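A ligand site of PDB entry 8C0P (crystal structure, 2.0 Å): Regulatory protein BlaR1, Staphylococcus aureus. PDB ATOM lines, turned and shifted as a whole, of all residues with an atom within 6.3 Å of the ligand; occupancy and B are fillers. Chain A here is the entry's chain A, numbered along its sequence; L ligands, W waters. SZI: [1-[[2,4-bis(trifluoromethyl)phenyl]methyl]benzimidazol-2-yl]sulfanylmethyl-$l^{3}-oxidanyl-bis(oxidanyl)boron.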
ATOM      1  N   PRO A  56      -7.105  19.784 -10.348  1.00  0.00           N
ATOM      2  CA  PRO A  56      -5.759  19.536  -9.820  1.00  0.00           C
ATOM      3  C   PRO A  56      -4.883  18.694 -10.741  1.00  0.00           C
ATOM      4  O   PRO A  56      -3.665  18.681 -10.598  1.00  0.00           O
ATOM      5  CB  PRO A  56      -6.068  18.825  -8.492  1.00  0.00           C
ATOM      6  CG  PRO A  56      -7.340  18.073  -8.771  1.00  0.00           C
ATOM      7  CD  PRO A  56      -8.143  19.006  -9.657  1.00  0.00           C
ATOM      8  N   ASN A  57      -5.507  17.957 -11.672  1.00  0.00           N
ATOM      9  CA  ASN A  57      -4.793  17.026 -12.541  1.00  0.00           C
ATOM     10  C   ASN A  57      -3.888  16.128 -11.685  1.00  0.00           C
ATOM     11  O   ASN A  57      -4.311  15.651 -10.625  1.00  0.00           O
ATOM     12  CB  ASN A  57      -4.108  17.795 -13.689  1.00  0.00           C
ATOM     13  CG  ASN A  57      -5.116  18.449 -14.611  1.00  0.00           C
ATOM     14  OD1 ASN A  57      -5.111  19.660 -14.799  1.00  0.00           O
ATOM     15  ND2 ASN A  57      -5.992  17.646 -15.187  1.00  0.00           N
ATOM     16  N   SER A  58      -2.643  15.892 -12.129  1.00  0.00           N
ATOM     17  CA  SER A  58      -1.810  14.926 -11.407  1.00  0.00           C
ATOM     18  C   SER A  58      -1.402  15.303  -9.983  1.00  0.00           C
ATOM     19  O   SER A  58      -0.857  14.464  -9.258  1.00  0.00           O
ATOM     20  CB  SER A  58      -0.528  14.650 -12.154  1.00  0.00           C
ATOM     21  OG  SER A  58      -0.831  13.989 -13.381  1.00  0.00           O
ATOM     22  N   THR A  59      -1.665  16.541  -9.545  1.00  0.00           N
ATOM     23  CA  THR A  59      -1.401  16.884  -8.154  1.00  0.00           C
ATOM     24  C   THR A  59      -2.284  16.053  -7.232  1.00  0.00           C
ATOM     25  O   THR A  59      -1.923  15.762  -6.087  1.00  0.00           O
ATOM     26  CB  THR A  59      -1.496  18.401  -7.892  1.00  0.00           C
ATOM     27  OG1 THR A  59      -2.845  18.846  -8.105  1.00  0.00           O
ATOM     28  CG2 THR A  59      -0.521  19.160  -8.758  1.00  0.00           C
ATOM     29  N   LYS A  61      -2.731  12.980  -7.426  1.00  0.00           N
ATOM     30  CA  LYS A  61      -2.105  11.693  -7.164  1.00  0.00           C
ATOM     31  C   LYS A  61      -1.496  11.619  -5.754  1.00  0.00           C
ATOM     32  O   LYS A  61      -1.318  10.532  -5.202  1.00  0.00           O
ATOM     33  CB  LYS A  61      -1.051  11.403  -8.232  1.00  0.00           C
ATOM     34  CG  LYS A  61      -1.601  11.170  -9.638  1.00  0.00           C
ATOM     35  CD  LYS A  61      -0.508  11.107 -10.659  1.00  0.00           C
ATOM     36  CE  LYS A  61      -0.899  10.425 -11.953  1.00  0.00           C
ATOM     37  NZ  LYS A  61      -1.318  11.380 -13.009  1.00  0.00           N
ATOM     38  N   PRO A  89       1.926   6.155 -25.119  1.00  0.00           N
ATOM     39  CA  PRO A  89       2.891   6.925 -25.901  1.00  0.00           C
ATOM     40  C   PRO A  89       4.122   7.449 -25.160  1.00  0.00           C
ATOM     41  O   PRO A  89       4.886   8.218 -25.735  1.00  0.00           O
ATOM     42  CB  PRO A  89       2.081   8.119 -26.437  1.00  0.00           C
ATOM     43  CG  PRO A  89       0.909   8.271 -25.481  1.00  0.00           C
ATOM     44  CD  PRO A  89       0.685   6.912 -24.856  1.00  0.00           C
ATOM     45  N   PHE A  90       4.300   7.034 -23.891  1.00  0.00           N
ATOM     46  CA  PHE A  90       5.466   7.375 -23.095  1.00  0.00           C
ATOM     47  C   PHE A  90       6.109   6.097 -22.569  1.00  0.00           C
ATOM     48  O   PHE A  90       5.454   5.296 -21.908  1.00  0.00           O
ATOM     49  CB  PHE A  90       5.056   8.309 -21.945  1.00  0.00           C
ATOM     50  CG  PHE A  90       4.161   9.449 -22.351  1.00  0.00           C
ATOM     51  CD1 PHE A  90       4.666  10.523 -23.068  1.00  0.00           C
ATOM     52  CD2 PHE A  90       2.794   9.417 -22.054  1.00  0.00           C
ATOM     53  CE1 PHE A  90       3.836  11.559 -23.455  1.00  0.00           C
ATOM     54  CE2 PHE A  90       1.969  10.463 -22.450  1.00  0.00           C
ATOM     55  CZ  PHE A  90       2.487  11.538 -23.148  1.00  0.00           C
ATOM     56  N   ALA A  92       8.144   5.473 -20.233  1.00  0.00           N
ATOM     57  CA  ALA A  92       8.181   5.320 -18.781  1.00  0.00           C
ATOM     58  C   ALA A  92       6.896   4.684 -18.238  1.00  0.00           C
ATOM     59  O   ALA A  92       6.896   4.124 -17.131  1.00  0.00           O
ATOM     60  CB  ALA A  92       8.445   6.657 -18.153  1.00  0.00           C
ATOM     61  N   TRP A  93       5.794   4.766 -19.003  1.00  0.00           N
ATOM     62  CA  TRP A  93       4.519   4.195 -18.594  1.00  0.00           C
ATOM     63  C   TRP A  93       4.451   2.711 -18.949  1.00  0.00           C
ATOM     64  O   TRP A  93       3.693   1.966 -18.334  1.00  0.00           O
ATOM     65  CB  TRP A  93       3.339   4.949 -19.238  1.00  0.00           C
ATOM     66  CG  TRP A  93       3.124   6.358 -18.766  1.00  0.00           C
ATOM     67  CD1 TRP A  93       3.968   7.136 -18.033  1.00  0.00           C
ATOM     68  CD2 TRP A  93       1.955   7.173 -19.003  1.00  0.00           C
ATOM     69  NE1 TRP A  93       3.426   8.373 -17.796  1.00  0.00           N
ATOM     70  CE2 TRP A  93       2.179   8.420 -18.383  1.00  0.00           C
ATOM     71  CE3 TRP A  93       0.756   6.973 -19.694  1.00  0.00           C
ATOM     72  CZ2 TRP A  93       1.246   9.451 -18.418  1.00  0.00           C
ATOM     73  CZ3 TRP A  93      -0.174   8.000 -19.719  1.00  0.00           C
ATOM     74  CH2 TRP A  93       0.074   9.221 -19.095  1.00  0.00           C
ATOM     75  N   GLN A 104       6.893   9.766  -9.849  1.00  0.00           N
ATOM     76  CA  GLN A 104       7.948  10.480 -10.557  1.00  0.00           C
ATOM     77  C   GLN A 104       7.566  10.690 -12.023  1.00  0.00           C
ATOM     78  O   GLN A 104       7.839  11.753 -12.582  1.00  0.00           O
ATOM     79  CB  GLN A 104       9.252   9.680 -10.457  1.00  0.00           C
ATOM     80  CG  GLN A 104      10.463  10.413 -10.998  1.00  0.00           C
ATOM     81  CD  GLN A 104      11.599   9.504 -11.404  1.00  0.00           C
ATOM     82  OE1 GLN A 104      11.526   8.278 -11.288  1.00  0.00           O
ATOM     83  NE2 GLN A 104      12.667  10.097 -11.905  1.00  0.00           N
ATOM     84  N   ASN A 105       6.951   9.670 -12.638  1.00  0.00           N
ATOM     85  CA  ASN A 105       6.683   9.677 -14.069  1.00  0.00           C
ATOM     86  C   ASN A 105       5.206   9.982 -14.358  1.00  0.00           C
ATOM     87  O   ASN A 105       4.796   9.935 -15.509  1.00  0.00           O
ATOM     88  CB  ASN A 105       7.162   8.362 -14.690  1.00  0.00           C
ATOM     89  CG  ASN A 105       8.666   8.255 -14.626  1.00  0.00           C
ATOM     90  OD1 ASN A 105       9.359   9.163 -15.074  1.00  0.00           O
ATOM     91  ND2 ASN A 105       9.180   7.195 -14.016  1.00  0.00           N
ATOM     92  N   SER A 106       4.434  10.315 -13.309  1.00  0.00           N
ATOM     93  CA  SER A 106       3.026  10.691 -13.450  1.00  0.00           C
ATOM     94  C   SER A 106       2.275   9.645 -14.286  1.00  0.00           C
ATOM     95  O   SER A 106       1.614   9.954 -15.274  1.00  0.00           O
ATOM     96  CB  SER A 106       2.900  12.081 -14.010  1.00  0.00           C
ATOM     97  OG  SER A 106       1.849  12.790 -13.358  1.00  0.00           O
ATOM     98  N   ASN A 108      -0.561   7.615 -15.105  1.00  0.00           N
ATOM     99  CA  ASN A 108      -1.987   7.679 -14.854  1.00  0.00           C
ATOM    100  C   ASN A 108      -2.544   6.304 -14.461  1.00  0.00           C
ATOM    101  O   ASN A 108      -3.374   6.208 -13.569  1.00  0.00           O
ATOM    102  CB  ASN A 108      -2.729   8.275 -16.057  1.00  0.00           C
ATOM    103  CG  ASN A 108      -2.399   9.739 -16.302  1.00  0.00           C
ATOM    104  OD1 ASN A 108      -1.687  10.364 -15.516  1.00  0.00           O
ATOM    105  ND2 ASN A 108      -2.924  10.287 -17.381  1.00  0.00           N
ATOM    106  N   MET A 145      -9.039  14.833 -13.361  1.00  0.00           N
ATOM    107  CA  MET A 145      -8.339  15.182 -14.598  1.00  0.00           C
ATOM    108  C   MET A 145      -9.270  15.988 -15.511  1.00  0.00           C
ATOM    109  O   MET A 145     -10.037  15.410 -16.285  1.00  0.00           O
ATOM    110  CB  MET A 145      -7.858  13.926 -15.332  1.00  0.00           C
ATOM    111  CG  MET A 145      -6.709  13.206 -14.644  1.00  0.00           C
ATOM    112  SD  MET A 145      -5.123  14.132 -14.569  1.00  0.00           S
ATOM    113  CE  MET A 145      -4.040  12.886 -13.872  1.00  0.00           C
ATOM    114  N   LYS A 195       4.984  17.774  -6.558  1.00  0.00           N
ATOM    115  CA  LYS A 195       4.292  17.052  -7.607  1.00  0.00           C
ATOM    116  C   LYS A 195       3.810  18.047  -8.650  1.00  0.00           C
ATOM    117  O   LYS A 195       3.138  19.038  -8.327  1.00  0.00           O
ATOM    118  CB  LYS A 195       3.093  16.290  -7.025  1.00  0.00           C
ATOM    119  CG  LYS A 195       2.354  15.396  -8.010  1.00  0.00           C
ATOM    120  CD  LYS A 195       3.232  14.295  -8.570  1.00  0.00           C
ATOM    121  CE  LYS A 195       2.618  13.502  -9.701  1.00  0.00           C
ATOM    122  NZ  LYS A 195       2.861  14.167 -11.002  1.00  0.00           N
ATOM    123  N   THR A 196       4.120  17.752  -9.917  1.00  0.00           N
ATOM    124  CA  THR A 196       3.593  18.513 -11.029  1.00  0.00           C
ATOM    125  C   THR A 196       2.183  18.036 -11.398  1.00  0.00           C
ATOM    126  O   THR A 196       1.783  16.906 -11.144  1.00  0.00           O
ATOM    127  CB  THR A 196       4.513  18.404 -12.244  1.00  0.00           C
ATOM    128  OG1 THR A 196       4.683  17.014 -12.530  1.00  0.00           O
ATOM    129  CG2 THR A 196       5.850  19.082 -12.013  1.00  0.00           C
ATOM    130  N   GLY A 197       1.436  18.950 -11.988  1.00  0.00           N
ATOM    131  CA  GLY A 197       0.222  18.586 -12.677  1.00  0.00           C
ATOM    132  C   GLY A 197       0.121  19.381 -13.967  1.00  0.00           C
ATOM    133  O   GLY A 197       0.501  20.547 -14.002  1.00  0.00           O
ATOM    134  N   THR A 198      -0.442  18.727 -14.987  1.00  0.00           N
ATOM    135  CA  THR A 198      -0.603  19.318 -16.298  1.00  0.00           C
ATOM    136  C   THR A 198      -1.956  18.899 -16.864  1.00  0.00           C
ATOM    137  O   THR A 198      -2.244  17.705 -16.934  1.00  0.00           O
ATOM    138  CB  THR A 198       0.492  18.862 -17.261  1.00  0.00           C
ATOM    139  OG1 THR A 198       1.771  19.274 -16.764  1.00  0.00           O
ATOM    140  CG2 THR A 198       0.297  19.403 -18.657  1.00  0.00           C
ATOM    141  N   GLY A 199      -2.765  19.882 -17.232  1.00  0.00           N
ATOM    142  CA  GLY A 199      -4.004  19.622 -17.954  1.00  0.00           C
ATOM    143  C   GLY A 199      -3.828  19.898 -19.439  1.00  0.00           C
ATOM    144  O   GLY A 199      -3.212  20.906 -19.804  1.00  0.00           O
ATOM    145  N   ILE A 200      -4.367  19.018 -20.282  1.00  0.00           N
ATOM    146  CA  ILE A 200      -4.342  19.208 -21.729  1.00  0.00           C
ATOM    147  C   ILE A 200      -5.776  19.240 -22.252  1.00  0.00           C
ATOM    148  O   ILE A 200      -6.542  18.310 -22.033  1.00  0.00           O
ATOM    149  CB  ILE A 200      -3.495  18.112 -22.410  1.00  0.00           C
ATOM    150  CG1 ILE A 200      -2.058  18.077 -21.879  1.00  0.00           C
ATOM    151  CG2 ILE A 200      -3.521  18.285 -23.925  1.00  0.00           C
ATOM    152  CD1 ILE A 200      -1.254  16.894 -22.367  1.00  0.00           C
ATOM    153  N   TYR A 205      -1.769  23.017 -23.614  1.00  0.00           N
ATOM    154  CA  TYR A 205      -1.638  23.164 -22.174  1.00  0.00           C
ATOM    155  C   TYR A 205      -2.665  24.161 -21.660  1.00  0.00           C
ATOM    156  O   TYR A 205      -2.727  25.299 -22.130  1.00  0.00           O
ATOM    157  CB  TYR A 205      -0.218  23.613 -21.818  1.00  0.00           C
ATOM    158  CG  TYR A 205       0.859  22.573 -22.031  1.00  0.00           C
ATOM    159  CD1 TYR A 205       0.634  21.247 -21.693  1.00  0.00           C
ATOM    160  CD2 TYR A 205       2.103  22.909 -22.536  1.00  0.00           C
ATOM    161  CE1 TYR A 205       1.608  20.277 -21.859  1.00  0.00           C
ATOM    162  CE2 TYR A 205       3.102  21.956 -22.693  1.00  0.00           C
ATOM    163  CZ  TYR A 205       2.847  20.634 -22.355  1.00  0.00           C
ATOM    164  OH  TYR A 205       3.795  19.648 -22.508  1.00  0.00           O
ATOM    165  N   SER A 233       2.062  24.615 -18.101  1.00  0.00           N
ATOM    166  CA  SER A 233       2.449  23.220 -17.914  1.00  0.00           C
ATOM    167  C   SER A 233       2.911  23.026 -16.478  1.00  0.00           C
ATOM    168  O   SER A 233       3.327  23.984 -15.834  1.00  0.00           O
ATOM    169  CB  SER A 233       3.526  22.814 -18.886  1.00  0.00           C
ATOM    170  OG  SER A 233       4.774  23.427 -18.539  1.00  0.00           O
ATOM    171  N   GLY A 234       2.862  21.772 -16.003  1.00  0.00           N
ATOM    172  CA  GLY A 234       3.442  21.386 -14.728  1.00  0.00           C
ATOM    173  C   GLY A 234       4.938  21.693 -14.647  1.00  0.00           C
ATOM    174  O   GLY A 234       5.417  22.187 -13.635  1.00  0.00           O
ATOM    175  N   LYS A 235       5.662  21.382 -15.729  1.00  0.00           N
ATOM    176  CA  LYS A 235       7.097  21.607 -15.768  1.00  0.00           C
ATOM    177  C   LYS A 235       7.416  23.096 -15.580  1.00  0.00           C
ATOM    178  O   LYS A 235       8.327  23.454 -14.841  1.00  0.00           O
ATOM    179  CB  LYS A 235       7.704  21.085 -17.077  1.00  0.00           C
ATOM    180  CG  LYS A 235       9.234  21.083 -17.095  1.00  0.00           C
ATOM    181  CD  LYS A 235       9.877  20.970 -18.457  1.00  0.00           C
ATOM    182  CE  LYS A 235      11.343  21.339 -18.399  1.00  0.00           C
ATOM    183  NZ  LYS A 235      12.046  20.934 -19.641  1.00  0.00           N
HETATM  184  O2  SZI L   1       0.926  15.076 -14.642  1.00  0.00           O
HETATM  185  C10 SZI L   1      -0.651  13.603 -18.683  1.00  0.00           C
HETATM  186  C11 SZI L   1       4.734  14.033 -19.650  1.00  0.00           C
HETATM  187  C12 SZI L   1       4.740  12.645 -19.540  1.00  0.00           C
HETATM  188  O1  SZI L   1      -1.250  15.906 -14.778  1.00  0.00           O
HETATM  189  C01 SZI L   1      -1.829  12.467 -20.114  1.00  0.00           C
HETATM  190  N01 SZI L   1      -1.667  12.760 -18.742  1.00  0.00           N
HETATM  191  S01 SZI L   1       0.061  14.375 -17.291  1.00  0.00           S
HETATM  192  C02 SZI L   1      -2.723  11.640 -20.793  1.00  0.00           C
HETATM  193  N02 SZI L   1      -0.133  13.855 -19.931  1.00  0.00           N
HETATM  194  C03 SZI L   1      -2.656  11.527 -22.173  1.00  0.00           C
HETATM  195  C04 SZI L   1      -1.698  12.214 -22.927  1.00  0.00           C
HETATM  196  C05 SZI L   1      -0.787  13.038 -22.266  1.00  0.00           C
HETATM  197  C06 SZI L   1      -0.865  13.148 -20.873  1.00  0.00           C
HETATM  198  C07 SZI L   1       1.001  14.733 -20.251  1.00  0.00           C
HETATM  199  C08 SZI L   1       2.336  14.048 -20.008  1.00  0.00           C
HETATM  200  C09 SZI L   1       3.559  14.765 -19.882  1.00  0.00           C
HETATM  201  C13 SZI L   1       3.545  11.957 -19.675  1.00  0.00           C
HETATM  202  C14 SZI L   1       2.371  12.643 -19.902  1.00  0.00           C
HETATM  203  C15 SZI L   1       3.602  16.294 -19.980  1.00  0.00           C
HETATM  204  C16 SZI L   1       6.035  11.929 -19.307  1.00  0.00           C
HETATM  205  C17 SZI L   1      -0.851  13.753 -15.852  1.00  0.00           C
HETATM  206  B   SZI L   1      -0.481  14.654 -14.627  1.00  0.00           B
HETATM  207  F01 SZI L   1       2.918  16.839 -20.999  1.00  0.00           F
HETATM  208  F02 SZI L   1       3.094  16.858 -18.876  1.00  0.00           F
HETATM  209  F03 SZI L   1       4.855  16.768 -20.106  1.00  0.00           F
HETATM  210  F17 SZI L   1       6.795  12.530 -18.390  1.00  0.00           F
HETATM  211  F18 SZI L   1       5.928  10.651 -18.900  1.00  0.00           F
HETATM  212  F19 SZI L   1       6.745  11.936 -20.437  1.00  0.00           F
HETATM  213  O   HOH W   1       4.518  19.476 -17.790  1.00  0.00           O
HETATM  214  O   HOH W   2       2.720  17.137 -14.958  1.00  0.00           O
HETATM  215  O   HOH W   3       3.950  14.805 -16.214  1.00  0.00           O
HETATM  216  O   HOH W   4      -4.142   8.929 -19.521  1.00  0.00           O
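Water W2 lies within hydrogen-bond range of O2 of the ligand (2.8 Å), OG1 of Thr 198 (3.0 Å) and OG1 of Thr 196 (3.1 Å).
Water W1 lies within hydrogen-bond range of OG1 of Thr 198 (2.9 Å), N of Lys 235 (3.0 Å) and N of Gly 234 (3.3 Å).
An oxygen (O2) of the ligand is in hydrogen-bond range of the side-chain hydroxyl (OG) of Ser 106 (2.8 Å).
The side-chain amide nitrogen of Asn 108 lies within hydrogen-bond range of a nitrogen (N01) of the ligand (3.1 Å).
N of Ser 58 sits at hydrogen-bond distance from O1 of the ligand, 3.0 Å away.
The backbone carbonyl oxygen (O) of Thr 198 sits at hydrogen-bond distance from an oxygen (O1) of the ligand (3.0 Å).
N of Thr 198 is in hydrogen-bond range of O1 of the ligand, at 2.9 Å.
OG of Ser 58 is bonded to B of the ligand, at 1.5 Å.
The side-chain hydroxyl of Tyr 205 sits close to a fluorine (F01) of the ligand, 3.3 Å away.
Asn 57 touches the ligand.
NZ of Lys 61 touches C17 of the ligand (3.7 Å).
Phe 90 touches the ligand (CE2 to C14, 3.4 Å).
Trp 93 touches the ligand (NE1 to F18, 3.6 Å).
Asn 105 touches the ligand.
CE of Met 145 touches C17 of the ligand, 3.9 Å away.
CA of Gly 197 touches O1 of the ligand, 3.7 Å away.
CD1 of Ile 200 touches C07 of the ligand, at 3.8 Å.
Hydrophobic or aromatic side chains that line the ligand: Phe 90, Trp 93, Met 145, Ile 200 and Tyr 205.
Within 4 Å of the ligand: Asn 57, Ser 58, Lys 61, Phe 90, Trp 93, Asn 105, Ser 106, Asn 108, Met 145, Gly 197, Thr 198, Ile 200 and Tyr 205.
N of Gly 199 lies close to OD1 of Asn 57, 3.4 Å away.
OG of Ser 106 is in hydrogen-bond range of NZ of Lys 61 (3.5 Å).
SD of Met 145 lies close to ND2 of Asn 57 (3.7 Å).
OG of Ser 58 lies within hydrogen-bond range of OG of Ser 106, at 2.9 Å.
OD1 of Asn 108 sits close to O of Ser 106 (3.3 Å).
OG1 of Thr 198 is in hydrogen-bond range of N of Gly 234, 2.8 Å away.
The side-chain amino group (NZ) of Lys 61 sits at hydrogen-bond distance from the side-chain hydroxyl (OG) of Ser 58 (2.7 Å).
OD1 of Asn 108 lies within hydrogen-bond range of NZ of Lys 61 (2.7 Å).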
